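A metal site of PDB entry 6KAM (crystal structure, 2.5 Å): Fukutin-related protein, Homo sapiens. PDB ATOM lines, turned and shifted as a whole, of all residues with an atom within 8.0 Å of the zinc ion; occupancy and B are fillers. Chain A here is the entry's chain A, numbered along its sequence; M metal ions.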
ATOM      1  N   ARG A 235     -32.086 -14.483  13.528  1.00  0.00           N
ATOM      2  CA  ARG A 235     -32.075 -15.911  13.825  1.00  0.00           C
ATOM      3  C   ARG A 235     -33.392 -16.415  14.388  1.00  0.00           C
ATOM      4  O   ARG A 235     -33.634 -17.642  14.382  1.00  0.00           O
ATOM      5  CB  ARG A 235     -30.961 -16.232  14.835  1.00  0.00           C
ATOM      6  CG  ARG A 235     -29.571 -15.881  14.377  1.00  0.00           C
ATOM      7  CD  ARG A 235     -28.942 -17.040  13.612  1.00  0.00           C
ATOM      8  NE  ARG A 235     -27.509 -16.854  13.481  1.00  0.00           N
ATOM      9  CZ  ARG A 235     -26.939 -16.081  12.550  1.00  0.00           C
ATOM     10  NH1 ARG A 235     -27.699 -15.440  11.683  1.00  0.00           N
ATOM     11  NH2 ARG A 235     -25.617 -15.957  12.503  1.00  0.00           N
ATOM     12  N   TRP A 246     -37.288 -20.354  13.819  1.00  0.00           N
ATOM     13  CA  TRP A 246     -35.841 -20.323  13.981  1.00  0.00           C
ATOM     14  C   TRP A 246     -35.133 -20.294  12.637  1.00  0.00           C
ATOM     15  O   TRP A 246     -35.595 -20.880  11.652  1.00  0.00           O
ATOM     16  CB  TRP A 246     -35.346 -21.518  14.807  1.00  0.00           C
ATOM     17  CG  TRP A 246     -35.821 -21.507  16.234  1.00  0.00           C
ATOM     18  CD1 TRP A 246     -36.873 -22.193  16.747  1.00  0.00           C
ATOM     19  CD2 TRP A 246     -35.280 -20.738  17.322  1.00  0.00           C
ATOM     20  NE1 TRP A 246     -37.020 -21.922  18.079  1.00  0.00           N
ATOM     21  CE2 TRP A 246     -36.048 -21.026  18.465  1.00  0.00           C
ATOM     22  CE3 TRP A 246     -34.210 -19.839  17.443  1.00  0.00           C
ATOM     23  CZ2 TRP A 246     -35.801 -20.448  19.722  1.00  0.00           C
ATOM     24  CZ3 TRP A 246     -33.958 -19.258  18.691  1.00  0.00           C
ATOM     25  CH2 TRP A 246     -34.750 -19.574  19.809  1.00  0.00           C
ATOM     26  N   PHE A 247     -33.999 -19.580  12.610  1.00  0.00           N
ATOM     27  CA  PHE A 247     -33.178 -19.470  11.415  1.00  0.00           C
ATOM     28  C   PHE A 247     -31.692 -19.499  11.779  1.00  0.00           C
ATOM     29  O   PHE A 247     -30.868 -18.895  11.092  1.00  0.00           O
ATOM     30  CB  PHE A 247     -33.513 -18.192  10.640  1.00  0.00           C
ATOM     31  CG  PHE A 247     -34.938 -18.152  10.154  1.00  0.00           C
ATOM     32  CD1 PHE A 247     -35.942 -17.622  10.943  1.00  0.00           C
ATOM     33  CD2 PHE A 247     -35.272 -18.676   8.912  1.00  0.00           C
ATOM     34  CE1 PHE A 247     -37.249 -17.599  10.489  1.00  0.00           C
ATOM     35  CE2 PHE A 247     -36.570 -18.656   8.461  1.00  0.00           C
ATOM     36  CZ  PHE A 247     -37.555 -18.113   9.242  1.00  0.00           C
ATOM     37  N   GLY A 248     -31.343 -20.216  12.854  1.00  0.00           N
ATOM     38  CA  GLY A 248     -29.964 -20.292  13.274  1.00  0.00           C
ATOM     39  C   GLY A 248     -29.388 -21.689  13.267  1.00  0.00           C
ATOM     40  O   GLY A 248     -29.647 -22.465  12.330  1.00  0.00           O
ATOM     41  N   CYS A 249     -28.601 -22.026  14.288  1.00  0.00           N
ATOM     42  CA  CYS A 249     -28.048 -23.361  14.407  1.00  0.00           C
ATOM     43  C   CYS A 249     -29.087 -24.301  15.019  1.00  0.00           C
ATOM     44  O   CYS A 249     -30.193 -23.887  15.381  1.00  0.00           O
ATOM     45  CB  CYS A 249     -26.749 -23.354  15.225  1.00  0.00           C
ATOM     46  SG  CYS A 249     -26.917 -22.865  16.964  1.00  0.00           S
ATOM     47  N   ASN A 250     -28.735 -25.582  15.127  1.00  0.00           N
ATOM     48  CA  ASN A 250     -29.570 -26.601  15.753  1.00  0.00           C
ATOM     49  C   ASN A 250     -28.717 -27.862  15.934  1.00  0.00           C
ATOM     50  O   ASN A 250     -27.490 -27.838  15.764  1.00  0.00           O
ATOM     51  CB  ASN A 250     -30.824 -26.905  14.933  1.00  0.00           C
ATOM     52  CG  ASN A 250     -30.507 -27.390  13.534  1.00  0.00           C
ATOM     53  OD1 ASN A 250     -29.956 -28.480  13.360  1.00  0.00           O
ATOM     54  ND2 ASN A 250     -30.839 -26.588  12.531  1.00  0.00           N
ATOM     55  N   THR A 253     -26.474 -28.818  12.777  1.00  0.00           N
ATOM     56  CA  THR A 253     -25.568 -27.881  12.152  1.00  0.00           C
ATOM     57  C   THR A 253     -24.352 -27.616  13.032  1.00  0.00           C
ATOM     58  O   THR A 253     -24.259 -28.089  14.167  1.00  0.00           O
ATOM     59  CB  THR A 253     -26.292 -26.568  11.857  1.00  0.00           C
ATOM     60  OG1 THR A 253     -26.371 -25.799  13.062  1.00  0.00           O
ATOM     61  CG2 THR A 253     -27.702 -26.833  11.351  1.00  0.00           C
ATOM     62  N   THR A 254     -23.408 -26.851  12.496  1.00  0.00           N
ATOM     63  CA  THR A 254     -22.397 -26.258  13.353  1.00  0.00           C
ATOM     64  C   THR A 254     -23.020 -25.120  14.173  1.00  0.00           C
ATOM     65  O   THR A 254     -24.101 -24.610  13.856  1.00  0.00           O
ATOM     66  CB  THR A 254     -21.224 -25.733  12.526  1.00  0.00           C
ATOM     67  OG1 THR A 254     -21.684 -24.694  11.660  1.00  0.00           O
ATOM     68  CG2 THR A 254     -20.627 -26.828  11.699  1.00  0.00           C
ATOM     69  N   ARG A 255     -22.330 -24.730  15.229  1.00  0.00           N
ATOM     70  CA  ARG A 255     -22.773 -23.544  15.948  1.00  0.00           C
ATOM     71  C   ARG A 255     -22.504 -22.306  15.091  1.00  0.00           C
ATOM     72  O   ARG A 255     -21.683 -22.314  14.172  1.00  0.00           O
ATOM     73  CB  ARG A 255     -22.103 -23.440  17.316  1.00  0.00           C
ATOM     74  CG  ARG A 255     -20.630 -23.120  17.306  1.00  0.00           C
ATOM     75  CD  ARG A 255     -20.083 -23.023  18.726  1.00  0.00           C
ATOM     76  NE  ARG A 255     -18.735 -22.474  18.740  1.00  0.00           N
ATOM     77  CZ  ARG A 255     -17.828 -22.721  19.684  1.00  0.00           C
ATOM     78  NH1 ARG A 255     -18.117 -23.534  20.700  1.00  0.00           N
ATOM     79  NH2 ARG A 255     -16.627 -22.175  19.604  1.00  0.00           N
ATOM     80  N   CYS A 256     -23.257 -21.238  15.391  1.00  0.00           N
ATOM     81  CA  CYS A 256     -23.225 -20.044  14.544  1.00  0.00           C
ATOM     82  C   CYS A 256     -21.841 -19.409  14.495  1.00  0.00           C
ATOM     83  O   CYS A 256     -21.409 -18.944  13.434  1.00  0.00           O
ATOM     84  CB  CYS A 256     -24.261 -19.030  15.034  1.00  0.00           C
ATOM     85  SG  CYS A 256     -25.996 -19.566  14.914  1.00  0.00           S
ATOM     86  N   PHE A 257     -21.130 -19.387  15.602  1.00  0.00           N
ATOM     87  CA  PHE A 257     -19.826 -18.731  15.666  1.00  0.00           C
ATOM     88  C   PHE A 257     -18.723 -19.769  15.740  1.00  0.00           C
ATOM     89  O   PHE A 257     -18.865 -20.797  16.408  1.00  0.00           O
ATOM     90  CB  PHE A 257     -19.747 -17.765  16.862  1.00  0.00           C
ATOM     91  CG  PHE A 257     -20.081 -18.388  18.198  1.00  0.00           C
ATOM     92  CD1 PHE A 257     -21.399 -18.649  18.553  1.00  0.00           C
ATOM     93  CD2 PHE A 257     -19.081 -18.690  19.106  1.00  0.00           C
ATOM     94  CE1 PHE A 257     -21.715 -19.215  19.778  1.00  0.00           C
ATOM     95  CE2 PHE A 257     -19.388 -19.259  20.334  1.00  0.00           C
ATOM     96  CZ  PHE A 257     -20.699 -19.521  20.668  1.00  0.00           C
ATOM     97  N   THR A 274     -24.943 -12.982  21.943  1.00  0.00           N
ATOM     98  CA  THR A 274     -24.981 -14.383  21.539  1.00  0.00           C
ATOM     99  C   THR A 274     -26.252 -14.658  20.736  1.00  0.00           C
ATOM    100  O   THR A 274     -27.335 -14.180  21.102  1.00  0.00           O
ATOM    101  CB  THR A 274     -24.907 -15.302  22.753  1.00  0.00           C
ATOM    102  OG1 THR A 274     -23.753 -14.969  23.532  1.00  0.00           O
ATOM    103  CG2 THR A 274     -24.797 -16.759  22.318  1.00  0.00           C
ATOM    104  N   PRO A 275     -26.148 -15.367  19.622  1.00  0.00           N
ATOM    105  CA  PRO A 275     -27.335 -15.726  18.838  1.00  0.00           C
ATOM    106  C   PRO A 275     -28.333 -16.496  19.673  1.00  0.00           C
ATOM    107  O   PRO A 275     -27.939 -17.336  20.496  1.00  0.00           O
ATOM    108  CB  PRO A 275     -26.759 -16.579  17.706  1.00  0.00           C
ATOM    109  CG  PRO A 275     -25.375 -16.034  17.529  1.00  0.00           C
ATOM    110  CD  PRO A 275     -24.900 -15.709  18.916  1.00  0.00           C
ATOM    111  N   PRO A 276     -29.631 -16.251  19.485  1.00  0.00           N
ATOM    112  CA  PRO A 276     -30.618 -16.894  20.359  1.00  0.00           C
ATOM    113  C   PRO A 276     -30.692 -18.412  20.177  1.00  0.00           C
ATOM    114  O   PRO A 276     -30.989 -19.123  21.137  1.00  0.00           O
ATOM    115  CB  PRO A 276     -31.935 -16.197  19.988  1.00  0.00           C
ATOM    116  CG  PRO A 276     -31.712 -15.646  18.632  1.00  0.00           C
ATOM    117  CD  PRO A 276     -30.251 -15.352  18.505  1.00  0.00           C
ATOM    118  N   CYS A 277     -30.404 -18.924  18.983  1.00  0.00           N
ATOM    119  CA  CYS A 277     -30.318 -20.371  18.809  1.00  0.00           C
ATOM    120  C   CYS A 277     -29.202 -20.954  19.664  1.00  0.00           C
ATOM    121  O   CYS A 277     -29.354 -22.056  20.218  1.00  0.00           O
ATOM    122  CB  CYS A 277     -30.086 -20.706  17.335  1.00  0.00           C
ATOM    123  SG  CYS A 277     -28.817 -19.636  16.601  1.00  0.00           S
ATOM    124  N   CYS A 278     -28.081 -20.230  19.770  1.00  0.00           N
ATOM    125  CA  CYS A 278     -26.942 -20.728  20.528  1.00  0.00           C
ATOM    126  C   CYS A 278     -27.241 -20.695  22.024  1.00  0.00           C
ATOM    127  O   CYS A 278     -26.815 -21.588  22.766  1.00  0.00           O
ATOM    128  CB  CYS A 278     -25.700 -19.908  20.192  1.00  0.00           C
ATOM    129  SG  CYS A 278     -24.988 -20.091  18.496  1.00  0.00           S
ATOM    130  N   LEU A 279     -27.987 -19.692  22.483  1.00  0.00           N
ATOM    131  CA  LEU A 279     -28.437 -19.678  23.876  1.00  0.00           C
ATOM    132  C   LEU A 279     -29.472 -20.763  24.142  1.00  0.00           C
ATOM    133  O   LEU A 279     -29.450 -21.409  25.195  1.00  0.00           O
ATOM    134  CB  LEU A 279     -29.002 -18.295  24.238  1.00  0.00           C
ATOM    135  CG  LEU A 279     -28.032 -17.122  24.333  1.00  0.00           C
ATOM    136  CD1 LEU A 279     -28.797 -15.834  24.555  1.00  0.00           C
ATOM    137  CD2 LEU A 279     -26.996 -17.301  25.426  1.00  0.00           C
ATOM    138  N   ARG A 280     -30.406 -20.973  23.196  1.00  0.00           N
ATOM    139  CA  ARG A 280     -31.408 -22.023  23.348  1.00  0.00           C
ATOM    140  C   ARG A 280     -30.752 -23.405  23.477  1.00  0.00           C
ATOM    141  O   ARG A 280     -31.156 -24.208  24.325  1.00  0.00           O
ATOM    142  CB  ARG A 280     -32.382 -22.003  22.167  1.00  0.00           C
ATOM    143  CG  ARG A 280     -33.556 -22.970  22.288  1.00  0.00           C
ATOM    144  CD  ARG A 280     -33.931 -23.563  20.932  1.00  0.00           C
ATOM    145  NE  ARG A 280     -32.816 -24.274  20.329  1.00  0.00           N
ATOM    146  CZ  ARG A 280     -32.442 -25.510  20.641  1.00  0.00           C
ATOM    147  NH1 ARG A 280     -33.104 -26.211  21.555  1.00  0.00           N
ATOM    148  NH2 ARG A 280     -31.395 -26.053  20.029  1.00  0.00           N
ATOM    149  N   ALA A 281     -29.742 -23.679  22.662  1.00  0.00           N
ATOM    150  CA  ALA A 281     -29.021 -24.944  22.769  1.00  0.00           C
ATOM    151  C   ALA A 281     -28.213 -25.036  24.049  1.00  0.00           C
ATOM    152  O   ALA A 281     -28.079 -26.118  24.620  1.00  0.00           O
ATOM    153  CB  ALA A 281     -28.118 -25.147  21.548  1.00  0.00           C
ATOM    154  N   ASN A 371     -22.469 -29.575  16.556  1.00  0.00           N
ATOM    155  CA  ASN A 371     -22.681 -28.280  17.192  1.00  0.00           C
ATOM    156  C   ASN A 371     -21.919 -28.272  18.517  1.00  0.00           C
ATOM    157  O   ASN A 371     -22.347 -28.891  19.498  1.00  0.00           O
ATOM    158  CB  ASN A 371     -24.171 -28.047  17.422  1.00  0.00           C
ATOM    159  CG  ASN A 371     -24.492 -26.621  17.814  1.00  0.00           C
ATOM    160  OD1 ASN A 371     -23.723 -25.965  18.532  1.00  0.00           O
ATOM    161  ND2 ASN A 371     -25.625 -26.106  17.336  1.00  0.00           N
ATOM    162  N   LEU A 373     -21.371 -26.083  20.883  1.00  0.00           N
ATOM    163  CA  LEU A 373     -21.799 -25.429  22.115  1.00  0.00           C
ATOM    164  C   LEU A 373     -21.747 -26.435  23.265  1.00  0.00           C
ATOM    165  O   LEU A 373     -22.264 -27.554  23.134  1.00  0.00           O
ATOM    166  CB  LEU A 373     -23.205 -24.860  21.943  1.00  0.00           C
ATOM    167  CG  LEU A 373     -23.335 -23.756  20.893  1.00  0.00           C
ATOM    168  CD1 LEU A 373     -24.787 -23.549  20.469  1.00  0.00           C
ATOM    169  CD2 LEU A 373     -22.715 -22.445  21.375  1.00  0.00           C
HETATM  170 ZN    ZN M   1     -26.695 -20.526  16.953  1.00  0.00          ZN
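Of the 21 residues printed, 4 come within 4 Å of the zinc ion.
The nearest printed residue that does not touch the zinc ion is Pro 275 (4.02 Å).
The zinc ion is bound by the side-chain sulfur (SG) of Cys 277 (2.3 Å), the side-chain sulfur (SG) of Cys 278 (2.3 Å), the side-chain sulfur (SG) of Cys 249 (2.3 Å) and the side-chain sulfur (SG) of Cys 256 (2.4 Å).
SG of Cys 256 lies close to NE of Arg 235 (3.4 Å).
The side-chain sulfur of Cys 249 sits close to the side-chain amide nitrogen of Asn 371, 3.5 Å away.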
